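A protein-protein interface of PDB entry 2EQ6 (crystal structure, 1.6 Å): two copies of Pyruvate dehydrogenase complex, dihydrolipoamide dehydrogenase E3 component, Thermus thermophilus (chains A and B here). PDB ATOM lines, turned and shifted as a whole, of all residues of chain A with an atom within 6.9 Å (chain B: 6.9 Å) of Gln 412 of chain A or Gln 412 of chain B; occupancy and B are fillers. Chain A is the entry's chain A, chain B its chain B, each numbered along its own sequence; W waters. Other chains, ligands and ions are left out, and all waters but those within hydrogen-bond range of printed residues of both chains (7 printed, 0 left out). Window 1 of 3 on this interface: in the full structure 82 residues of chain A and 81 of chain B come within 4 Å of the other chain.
Of the printed residues of chain B, Gln 412 of chain A touches Gln 412. Gln 412 of chain B touches just one residue of chain A: Gln 412 (3.2 Å). Of the printed residues of chain B, Glu 415 of chain A touches Leu 416 and Leu 443. Printed residues of chain A within 4 Å of Leu 443 of chain B: Glu 415. Printed residues of chain A within 4 Å of Leu 416 of chain B: Glu 415. Of the printed residues of chain B, Leu 443 of chain A touches Glu 415. Of the printed residues of chain B, Leu 416 of chain A touches Glu 415 (3.6 Å). The nearest residue of chain A that does not touch Gln 412 of chain B is Glu 415 of chain A (5.0 Å). The nearest printed residue of chain B that does not touch Leu 443 of chain A is Gln 412 of chain B (5.6 Å).
Among the printed residues, merely in contact across the chains: Leu 416 of chain A with Glu 415 of chain B (3.6 Å) and Glu 415 of chain A with Leu 416 of chain B (3.6 Å).
Gln 412 of chain B touches its own counterpart, Gln 412 of chain A. Glu 415 of chain A touches Leu 416 of chain B, and with the chains exchanged Leu 416 of chain A touches Glu 415 of chain B. Glu 415 of chain A touches Leu 443 of chain B, and with the chains exchanged Leu 443 of chain A touches Glu 415 of chain B. Of the 5 pairs that touch across the chains among the printed residues, 5 have their exchanged pair printed and touching as well.
Hydrophobic or aromatic side chains of chain A within 4 Å of the printed part of chain B: Leu 416 and Leu 443. Of the 16 printed residues of chain B, 4 touch a printed residue of chain A. Printed residues of chain B that touch a printed residue of chain A: Gln 412, Glu 415, Leu 416 and Leu 443. Among the printed residues, no Asp or Glu carboxylate lies within 4 Å of a Lys or Arg side-chain nitrogen of the other chain.
The side-chain amide oxygen (OE1) of Gln 412 of chain A sits close to the side-chain amide oxygen (OE1) of Gln 412 of chain B. N of Leu 443 of chain A lies within hydrogen-bond range of OE1 of Glu 415 of chain B, 2.8 Å away. The side-chain carboxylate of Glu 415 of chain A lies within hydrogen-bond range of the backbone NH of Leu 443 of chain B, at 2.8 Å.
Water W6 bridges OE2 of Glu 351 of chain B and NH2 of Arg 381 of chain A. Water W5 lies within hydrogen-bond range of OE2 of Glu 351 of chain A and NH2 of Arg 381 of chain B. Water W1 bridges the side-chain carboxylate (OE2) of Glu 351 of chain A (2.6 Å) and the guanidinium group (NH2) of Arg 381 of chain B (3.3 Å). Water W2 bridges the side-chain carboxylate (OE2) of Glu 351 of chain B and the guanidinium group (NH2) of Arg 381 of chain A. Water W3 lies within hydrogen-bond range of the side-chain carboxylate (OE1) of Glu 415 of chain A (2.7 Å) and the guanidinium group (NE) of Arg 381 of chain B (2.8 Å). Water W7 lies within hydrogen-bond range of NE of Arg 381 of chain A (2.7 Å) and OE1 of Glu 415 of chain B (2.7 Å).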
ATOM      1  N   THR A 348       6.948 -32.189 -39.054  1.00  0.00           N
ATOM      2  CA  THR A 348       6.027 -33.165 -39.603  1.00  0.00           C
ATOM      3  C   THR A 348       4.843 -33.195 -38.637  1.00  0.00           C
ATOM      4  O   THR A 348       4.842 -32.492 -37.626  1.00  0.00           O
ATOM      5  CB  THR A 348       6.666 -34.555 -39.588  1.00  0.00           C
ATOM      6  OG1 THR A 348       7.365 -34.739 -38.345  1.00  0.00           O
ATOM      7  CG2 THR A 348       7.644 -34.707 -40.731  1.00  0.00           C
ATOM      8  N   PRO A 350       2.823 -36.186 -36.676  1.00  0.00           N
ATOM      9  CA  PRO A 350       3.195 -35.418 -35.484  1.00  0.00           C
ATOM     10  C   PRO A 350       4.581 -34.791 -35.597  1.00  0.00           C
ATOM     11  O   PRO A 350       5.410 -35.233 -36.395  1.00  0.00           O
ATOM     12  CB  PRO A 350       3.152 -36.469 -34.384  1.00  0.00           C
ATOM     13  CG  PRO A 350       3.683 -37.673 -35.093  1.00  0.00           C
ATOM     14  CD  PRO A 350       2.920 -37.634 -36.405  1.00  0.00           C
ATOM     15  N   GLU A 351       4.821 -33.755 -34.798  1.00  0.00           N
ATOM     16  CA  GLU A 351       6.117 -33.089 -34.783  1.00  0.00           C
ATOM     17  C   GLU A 351       7.053 -33.873 -33.870  1.00  0.00           C
ATOM     18  O   GLU A 351       6.609 -34.694 -33.063  1.00  0.00           O
ATOM     19  CB  GLU A 351       5.982 -31.660 -34.237  1.00  0.00           C
ATOM     20  CG  GLU A 351       5.138 -30.745 -35.106  1.00  0.00           C
ATOM     21  CD  GLU A 351       5.121 -29.304 -34.622  1.00  0.00           C
ATOM     22  OE1 GLU A 351       5.810 -28.978 -33.629  1.00  0.00           O
ATOM     23  OE2 GLU A 351       4.412 -28.490 -35.247  1.00  0.00           O
ATOM     24  N   ALA A 353      10.641 -33.211 -31.406  1.00  0.00           N
ATOM     25  CA  ALA A 353      11.516 -32.179 -30.872  1.00  0.00           C
ATOM     26  C   ALA A 353      12.396 -32.788 -29.800  1.00  0.00           C
ATOM     27  O   ALA A 353      11.984 -33.714 -29.100  1.00  0.00           O
ATOM     28  CB  ALA A 353      10.693 -31.032 -30.299  1.00  0.00           C
ATOM     29  N   ARG A 381      -6.192 -33.066 -23.455  1.00  0.00           N
ATOM     30  CA  ARG A 381      -6.089 -32.059 -24.506  1.00  0.00           C
ATOM     31  C   ARG A 381      -5.909 -32.714 -25.876  1.00  0.00           C
ATOM     32  O   ARG A 381      -6.541 -32.314 -26.851  1.00  0.00           O
ATOM     33  CB  ARG A 381      -4.913 -31.113 -24.223  1.00  0.00           C
ATOM     34  CG  ARG A 381      -4.777 -29.957 -25.218  1.00  0.00           C
ATOM     35  CD  ARG A 381      -6.094 -29.216 -25.382  1.00  0.00           C
ATOM     36  NE  ARG A 381      -5.960 -27.952 -26.106  1.00  0.00           N
ATOM     37  CZ  ARG A 381      -6.923 -27.418 -26.850  1.00  0.00           C
ATOM     38  NH1 ARG A 381      -8.082 -28.049 -26.982  1.00  0.00           N
ATOM     39  NH2 ARG A 381      -6.740 -26.243 -27.439  1.00  0.00           N
ATOM     40  N   LEU A 385      -8.356 -32.384 -29.445  1.00  0.00           N
ATOM     41  CA  LEU A 385      -7.792 -31.903 -30.705  1.00  0.00           C
ATOM     42  C   LEU A 385      -7.938 -32.989 -31.770  1.00  0.00           C
ATOM     43  O   LEU A 385      -7.356 -32.899 -32.851  1.00  0.00           O
ATOM     44  CB  LEU A 385      -6.307 -31.554 -30.528  1.00  0.00           C
ATOM     45  CG  LEU A 385      -5.968 -30.383 -29.601  1.00  0.00           C
ATOM     46  CD1 LEU A 385      -4.455 -30.267 -29.459  1.00  0.00           C
ATOM     47  CD2 LEU A 385      -6.552 -29.092 -30.158  1.00  0.00           C
ATOM     48  N   ILE A 408      10.223 -35.206 -27.494  1.00  0.00           N
ATOM     49  CA  ILE A 408       8.787 -35.179 -27.679  1.00  0.00           C
ATOM     50  C   ILE A 408       8.355 -35.513 -29.094  1.00  0.00           C
ATOM     51  O   ILE A 408       8.942 -35.030 -30.058  1.00  0.00           O
ATOM     52  CB  ILE A 408       8.243 -33.765 -27.376  1.00  0.00           C
ATOM     53  CG1 ILE A 408       8.744 -33.273 -26.018  1.00  0.00           C
ATOM     54  CG2 ILE A 408       6.721 -33.770 -27.421  1.00  0.00           C
ATOM     55  CD1 ILE A 408       8.410 -31.807 -25.754  1.00  0.00           C
ATOM     56  N   GLY A 410       4.682 -35.620 -31.155  1.00  0.00           N
ATOM     57  CA  GLY A 410       3.261 -35.343 -31.071  1.00  0.00           C
ATOM     58  C   GLY A 410       2.954 -33.937 -31.553  1.00  0.00           C
ATOM     59  O   GLY A 410       3.853 -33.218 -31.993  1.00  0.00           O
ATOM     60  N   PRO A 411       1.685 -33.514 -31.492  1.00  0.00           N
ATOM     61  CA  PRO A 411       1.327 -32.168 -31.938  1.00  0.00           C
ATOM     62  C   PRO A 411       2.027 -31.089 -31.109  1.00  0.00           C
ATOM     63  O   PRO A 411       2.204 -31.241 -29.899  1.00  0.00           O
ATOM     64  CB  PRO A 411      -0.194 -32.141 -31.772  1.00  0.00           C
ATOM     65  CG  PRO A 411      -0.429 -33.094 -30.632  1.00  0.00           C
ATOM     66  CD  PRO A 411       0.516 -34.228 -30.951  1.00  0.00           C
ATOM     67  N   GLN A 412       2.448 -30.024 -31.782  1.00  0.00           N
ATOM     68  CA  GLN A 412       3.103 -28.890 -31.137  1.00  0.00           C
ATOM     69  C   GLN A 412       4.392 -29.214 -30.382  1.00  0.00           C
ATOM     70  O   GLN A 412       4.807 -28.453 -29.511  1.00  0.00           O
ATOM     71  CB  GLN A 412       2.117 -28.209 -30.181  1.00  0.00           C
ATOM     72  CG  GLN A 412       0.775 -27.866 -30.819  1.00  0.00           C
ATOM     73  CD  GLN A 412       0.897 -26.852 -31.941  1.00  0.00           C
ATOM     74  OE1 GLN A 412       0.057 -26.799 -32.842  1.00  0.00           O
ATOM     75  NE2 GLN A 412       1.935 -26.029 -31.883  1.00  0.00           N
ATOM     76  N   ALA A 413       5.034 -30.328 -30.713  1.00  0.00           N
ATOM     77  CA  ALA A 413       6.272 -30.692 -30.026  1.00  0.00           C
ATOM     78  C   ALA A 413       7.293 -29.553 -30.073  1.00  0.00           C
ATOM     79  O   ALA A 413       7.978 -29.285 -29.092  1.00  0.00           O
ATOM     80  CB  ALA A 413       6.866 -31.951 -30.644  1.00  0.00           C
ATOM     81  N   GLY A 414       7.380 -28.883 -31.219  1.00  0.00           N
ATOM     82  CA  GLY A 414       8.327 -27.793 -31.373  1.00  0.00           C
ATOM     83  C   GLY A 414       8.069 -26.589 -30.486  1.00  0.00           C
ATOM     84  O   GLY A 414       8.994 -25.836 -30.184  1.00  0.00           O
ATOM     85  N   GLU A 415       6.819 -26.392 -30.079  1.00  0.00           N
ATOM     86  CA  GLU A 415       6.480 -25.264 -29.214  1.00  0.00           C
ATOM     87  C   GLU A 415       6.703 -25.623 -27.750  1.00  0.00           C
ATOM     88  O   GLU A 415       6.928 -24.744 -26.919  1.00  0.00           O
ATOM     89  CB  GLU A 415       5.018 -24.853 -29.409  1.00  0.00           C
ATOM     90  CG  GLU A 415       4.674 -24.430 -30.822  1.00  0.00           C
ATOM     91  CD  GLU A 415       5.316 -23.111 -31.223  1.00  0.00           C
ATOM     92  OE1 GLU A 415       5.146 -22.707 -32.393  1.00  0.00           O
ATOM     93  OE2 GLU A 415       5.979 -22.476 -30.371  1.00  0.00           O
ATOM     94  N   LEU A 416       6.639 -26.911 -27.436  1.00  0.00           N
ATOM     95  CA  LEU A 416       6.816 -27.371 -26.064  1.00  0.00           C
ATOM     96  C   LEU A 416       8.271 -27.557 -25.647  1.00  0.00           C
ATOM     97  O   LEU A 416       8.595 -27.526 -24.456  1.00  0.00           O
ATOM     98  CB  LEU A 416       6.088 -28.702 -25.857  1.00  0.00           C
ATOM     99  CG  LEU A 416       4.615 -28.771 -26.261  1.00  0.00           C
ATOM    100  CD1 LEU A 416       4.087 -30.171 -25.958  1.00  0.00           C
ATOM    101  CD2 LEU A 416       3.808 -27.717 -25.514  1.00  0.00           C
ATOM    102  N   ILE A 417       9.151 -27.748 -26.622  1.00  0.00           N
ATOM    103  CA  ILE A 417      10.546 -27.997 -26.312  1.00  0.00           C
ATOM    104  C   ILE A 417      11.287 -26.806 -25.698  1.00  0.00           C
ATOM    105  O   ILE A 417      12.295 -26.996 -25.007  1.00  0.00           O
ATOM    106  CB  ILE A 417      11.299 -28.535 -27.564  1.00  0.00           C
ATOM    107  CG1 ILE A 417      12.506 -29.372 -27.126  1.00  0.00           C
ATOM    108  CG2 ILE A 417      11.713 -27.386 -28.479  1.00  0.00           C
ATOM    109  CD1 ILE A 417      12.123 -30.676 -26.428  1.00  0.00           C
ATOM    110  N   LEU A 443      -1.249 -29.553 -23.937  1.00  0.00           N
ATOM    111  CA  LEU A 443      -0.315 -30.592 -24.318  1.00  0.00           C
ATOM    112  C   LEU A 443       0.934 -30.456 -23.446  1.00  0.00           C
ATOM    113  O   LEU A 443       1.612 -31.443 -23.185  1.00  0.00           O
ATOM    114  CB  LEU A 443       0.050 -30.451 -25.799  1.00  0.00           C
ATOM    115  CG  LEU A 443      -1.093 -30.695 -26.792  1.00  0.00           C
ATOM    116  CD1 LEU A 443      -0.646 -30.286 -28.187  1.00  0.00           C
ATOM    117  CD2 LEU A 443      -1.501 -32.163 -26.770  1.00  0.00           C
ATOM    118  N   THR B 348      -9.934 -19.345 -26.639  1.00  0.00           N
ATOM    119  CA  THR B 348     -10.496 -18.724 -27.825  1.00  0.00           C
ATOM    120  C   THR B 348      -9.369 -18.715 -28.858  1.00  0.00           C
ATOM    121  O   THR B 348      -8.248 -19.140 -28.570  1.00  0.00           O
ATOM    122  CB  THR B 348     -10.856 -17.269 -27.533  1.00  0.00           C
ATOM    123  OG1 THR B 348      -9.794 -16.670 -26.776  1.00  0.00           O
ATOM    124  CG2 THR B 348     -12.146 -17.179 -26.744  1.00  0.00           C
ATOM    125  N   PRO B 350      -7.613 -15.897 -31.270  1.00  0.00           N
ATOM    126  CA  PRO B 350      -6.377 -16.329 -30.613  1.00  0.00           C
ATOM    127  C   PRO B 350      -6.602 -16.645 -29.136  1.00  0.00           C
ATOM    128  O   PRO B 350      -7.585 -16.208 -28.545  1.00  0.00           O
ATOM    129  CB  PRO B 350      -5.464 -15.124 -30.796  1.00  0.00           C
ATOM    130  CG  PRO B 350      -6.422 -13.988 -30.679  1.00  0.00           C
ATOM    131  CD  PRO B 350      -7.569 -14.449 -31.548  1.00  0.00           C
ATOM    132  N   GLU B 351      -5.685 -17.406 -28.552  1.00  0.00           N
ATOM    133  CA  GLU B 351      -5.781 -17.759 -27.143  1.00  0.00           C
ATOM    134  C   GLU B 351      -5.178 -16.628 -26.329  1.00  0.00           C
ATOM    135  O   GLU B 351      -4.470 -15.775 -26.861  1.00  0.00           O
ATOM    136  CB  GLU B 351      -4.995 -19.044 -26.854  1.00  0.00           C
ATOM    137  CG  GLU B 351      -5.489 -20.252 -27.632  1.00  0.00           C
ATOM    138  CD  GLU B 351      -4.775 -21.543 -27.276  1.00  0.00           C
ATOM    139  OE1 GLU B 351      -3.839 -21.529 -26.443  1.00  0.00           O
ATOM    140  OE2 GLU B 351      -5.156 -22.585 -27.845  1.00  0.00           O
ATOM    141  N   ALA B 353      -3.211 -16.064 -22.443  1.00  0.00           N
ATOM    142  CA  ALA B 353      -2.645 -16.770 -21.305  1.00  0.00           C
ATOM    143  C   ALA B 353      -1.848 -15.794 -20.468  1.00  0.00           C
ATOM    144  O   ALA B 353      -1.288 -14.825 -20.988  1.00  0.00           O
ATOM    145  CB  ALA B 353      -1.751 -17.916 -21.774  1.00  0.00           C
ATOM    146  N   ARG B 381       6.934 -17.664 -37.990  1.00  0.00           N
ATOM    147  CA  ARG B 381       6.083 -18.831 -37.783  1.00  0.00           C
ATOM    148  C   ARG B 381       4.606 -18.462 -37.891  1.00  0.00           C
ATOM    149  O   ARG B 381       3.833 -19.154 -38.550  1.00  0.00           O
ATOM    150  CB  ARG B 381       6.362 -19.469 -36.418  1.00  0.00           C
ATOM    151  CG  ARG B 381       5.577 -20.758 -36.169  1.00  0.00           C
ATOM    152  CD  ARG B 381       5.750 -21.749 -37.318  1.00  0.00           C
ATOM    153  NE  ARG B 381       5.260 -23.090 -36.994  1.00  0.00           N
ATOM    154  CZ  ARG B 381       4.745 -23.936 -37.884  1.00  0.00           C
ATOM    155  NH1 ARG B 381       4.633 -23.582 -39.158  1.00  0.00           N
ATOM    156  NH2 ARG B 381       4.364 -25.147 -37.507  1.00  0.00           N
ATOM    157  N   LEU B 385       1.572 -19.952 -40.566  1.00  0.00           N
ATOM    158  CA  LEU B 385       0.354 -20.561 -40.045  1.00  0.00           C
ATOM    159  C   LEU B 385      -0.882 -19.854 -40.603  1.00  0.00           C
ATOM    160  O   LEU B 385      -2.003 -20.093 -40.155  1.00  0.00           O
ATOM    161  CB  LEU B 385       0.341 -20.514 -38.512  1.00  0.00           C
ATOM    162  CG  LEU B 385       1.406 -21.366 -37.815  1.00  0.00           C
ATOM    163  CD1 LEU B 385       1.326 -21.154 -36.309  1.00  0.00           C
ATOM    164  CD2 LEU B 385       1.204 -22.838 -38.158  1.00  0.00           C
ATOM    165  N   ILE B 408       0.317 -13.454 -22.832  1.00  0.00           N
ATOM    166  CA  ILE B 408       0.358 -13.801 -24.238  1.00  0.00           C
ATOM    167  C   ILE B 408      -1.012 -13.851 -24.887  1.00  0.00           C
ATOM    168  O   ILE B 408      -1.979 -14.322 -24.289  1.00  0.00           O
ATOM    169  CB  ILE B 408       0.988 -15.197 -24.417  1.00  0.00           C
ATOM    170  CG1 ILE B 408       2.329 -15.273 -23.688  1.00  0.00           C
ATOM    171  CG2 ILE B 408       1.145 -15.513 -25.903  1.00  0.00           C
ATOM    172  CD1 ILE B 408       2.900 -16.676 -23.626  1.00  0.00           C
ATOM    173  N   GLY B 410      -2.484 -14.965 -28.722  1.00  0.00           N
ATOM    174  CA  GLY B 410      -2.159 -15.483 -30.038  1.00  0.00           C
ATOM    175  C   GLY B 410      -2.355 -16.986 -30.071  1.00  0.00           C
ATOM    176  O   GLY B 410      -2.771 -17.579 -29.077  1.00  0.00           O
ATOM    177  N   PRO B 411      -2.080 -17.637 -31.205  1.00  0.00           N
ATOM    178  CA  PRO B 411      -2.261 -19.089 -31.248  1.00  0.00           C
ATOM    179  C   PRO B 411      -1.311 -19.786 -30.275  1.00  0.00           C
ATOM    180  O   PRO B 411      -0.187 -19.327 -30.058  1.00  0.00           O
ATOM    181  CB  PRO B 411      -1.961 -19.432 -32.709  1.00  0.00           C
ATOM    182  CG  PRO B 411      -0.983 -18.361 -33.111  1.00  0.00           C
ATOM    183  CD  PRO B 411      -1.568 -17.120 -32.484  1.00  0.00           C
ATOM    184  N   GLN B 412      -1.786 -20.872 -29.672  1.00  0.00           N
ATOM    185  CA  GLN B 412      -0.995 -21.673 -28.739  1.00  0.00           C
ATOM    186  C   GLN B 412      -0.518 -20.942 -27.486  1.00  0.00           C
ATOM    187  O   GLN B 412       0.411 -21.400 -26.821  1.00  0.00           O
ATOM    188  CB  GLN B 412       0.221 -22.264 -29.463  1.00  0.00           C
ATOM    189  CG  GLN B 412      -0.128 -23.002 -30.754  1.00  0.00           C
ATOM    190  CD  GLN B 412      -0.998 -24.216 -30.512  1.00  0.00           C
ATOM    191  OE1 GLN B 412      -1.769 -24.628 -31.381  1.00  0.00           O
ATOM    192  NE2 GLN B 412      -0.869 -24.811 -29.333  1.00  0.00           N
ATOM    193  N   ALA B 413      -1.146 -19.817 -27.152  1.00  0.00           N
ATOM    194  CA  ALA B 413      -0.737 -19.071 -25.961  1.00  0.00           C
ATOM    195  C   ALA B 413      -0.718 -19.968 -24.726  1.00  0.00           C
ATOM    196  O   ALA B 413       0.182 -19.877 -23.890  1.00  0.00           O
ATOM    197  CB  ALA B 413      -1.678 -17.888 -25.729  1.00  0.00           C
ATOM    198  N   GLY B 414      -1.724 -20.834 -24.621  1.00  0.00           N
ATOM    199  CA  GLY B 414      -1.822 -21.726 -23.484  1.00  0.00           C
ATOM    200  C   GLY B 414      -0.687 -22.718 -23.355  1.00  0.00           C
ATOM    201  O   GLY B 414      -0.382 -23.163 -22.251  1.00  0.00           O
ATOM    202  N   GLU B 415      -0.066 -23.085 -24.471  1.00  0.00           N
ATOM    203  CA  GLU B 415       1.044 -24.031 -24.420  1.00  0.00           C
ATOM    204  C   GLU B 415       2.327 -23.292 -24.052  1.00  0.00           C
ATOM    205  O   GLU B 415       3.166 -23.809 -23.311  1.00  0.00           O
ATOM    206  CB  GLU B 415       1.220 -24.732 -25.771  1.00  0.00           C
ATOM    207  CG  GLU B 415      -0.011 -25.493 -26.246  1.00  0.00           C
ATOM    208  CD  GLU B 415      -0.324 -26.717 -25.401  1.00  0.00           C
ATOM    209  OE1 GLU B 415      -1.362 -27.361 -25.671  1.00  0.00           O
ATOM    210  OE2 GLU B 415       0.462 -27.037 -24.478  1.00  0.00           O
ATOM    211  N   LEU B 416       2.462 -22.069 -24.554  1.00  0.00           N
ATOM    212  CA  LEU B 416       3.649 -21.262 -24.302  1.00  0.00           C
ATOM    213  C   LEU B 416       3.772 -20.737 -22.874  1.00  0.00           C
ATOM    214  O   LEU B 416       4.878 -20.480 -22.396  1.00  0.00           O
ATOM    215  CB  LEU B 416       3.683 -20.070 -25.266  1.00  0.00           C
ATOM    216  CG  LEU B 416       3.575 -20.361 -26.769  1.00  0.00           C
ATOM    217  CD1 LEU B 416       3.744 -19.055 -27.551  1.00  0.00           C
ATOM    218  CD2 LEU B 416       4.634 -21.369 -27.184  1.00  0.00           C
ATOM    219  N   ILE B 417       2.645 -20.582 -22.187  1.00  0.00           N
ATOM    220  CA  ILE B 417       2.672 -20.034 -20.839  1.00  0.00           C
ATOM    221  C   ILE B 417       3.345 -20.953 -19.811  1.00  0.00           C
ATOM    222  O   ILE B 417       3.789 -20.487 -18.766  1.00  0.00           O
ATOM    223  CB  ILE B 417       1.238 -19.626 -20.383  1.00  0.00           C
ATOM    224  CG1 ILE B 417       1.319 -18.530 -19.310  1.00  0.00           C
ATOM    225  CG2 ILE B 417       0.477 -20.833 -19.873  1.00  0.00           C
ATOM    226  CD1 ILE B 417       1.841 -17.189 -19.842  1.00  0.00           C
ATOM    227  N   LEU B 443       6.358 -20.205 -32.482  1.00  0.00           N
ATOM    228  CA  LEU B 443       5.674 -19.118 -31.806  1.00  0.00           C
ATOM    229  C   LEU B 443       6.379 -18.876 -30.468  1.00  0.00           C
ATOM    230  O   LEU B 443       6.407 -17.751 -29.978  1.00  0.00           O
ATOM    231  CB  LEU B 443       4.207 -19.490 -31.575  1.00  0.00           C
ATOM    232  CG  LEU B 443       3.389 -19.677 -32.856  1.00  0.00           C
ATOM    233  CD1 LEU B 443       2.070 -20.363 -32.536  1.00  0.00           C
ATOM    234  CD2 LEU B 443       3.157 -18.324 -33.524  1.00  0.00           C
HETATM  235  O   HOH W   1       4.299 -28.393 -37.867  1.00  0.00           O
HETATM  236  O   HOH W   2      -7.677 -23.226 -28.325  1.00  0.00           O
HETATM  237  O   HOH W   3       6.052 -24.033 -34.524  1.00  0.00           O
HETATM  238  O   HOH W   4      -2.800 -27.505 -31.037  1.00  0.00           O
HETATM  239  O   HOH W   5       3.494 -26.162 -35.050  1.00  0.00           O
HETATM  240  O   HOH W   6      -4.425 -24.923 -28.276  1.00  0.00           O
HETATM  241  O   HOH W   7      -3.885 -26.478 -25.275  1.00  0.00           O
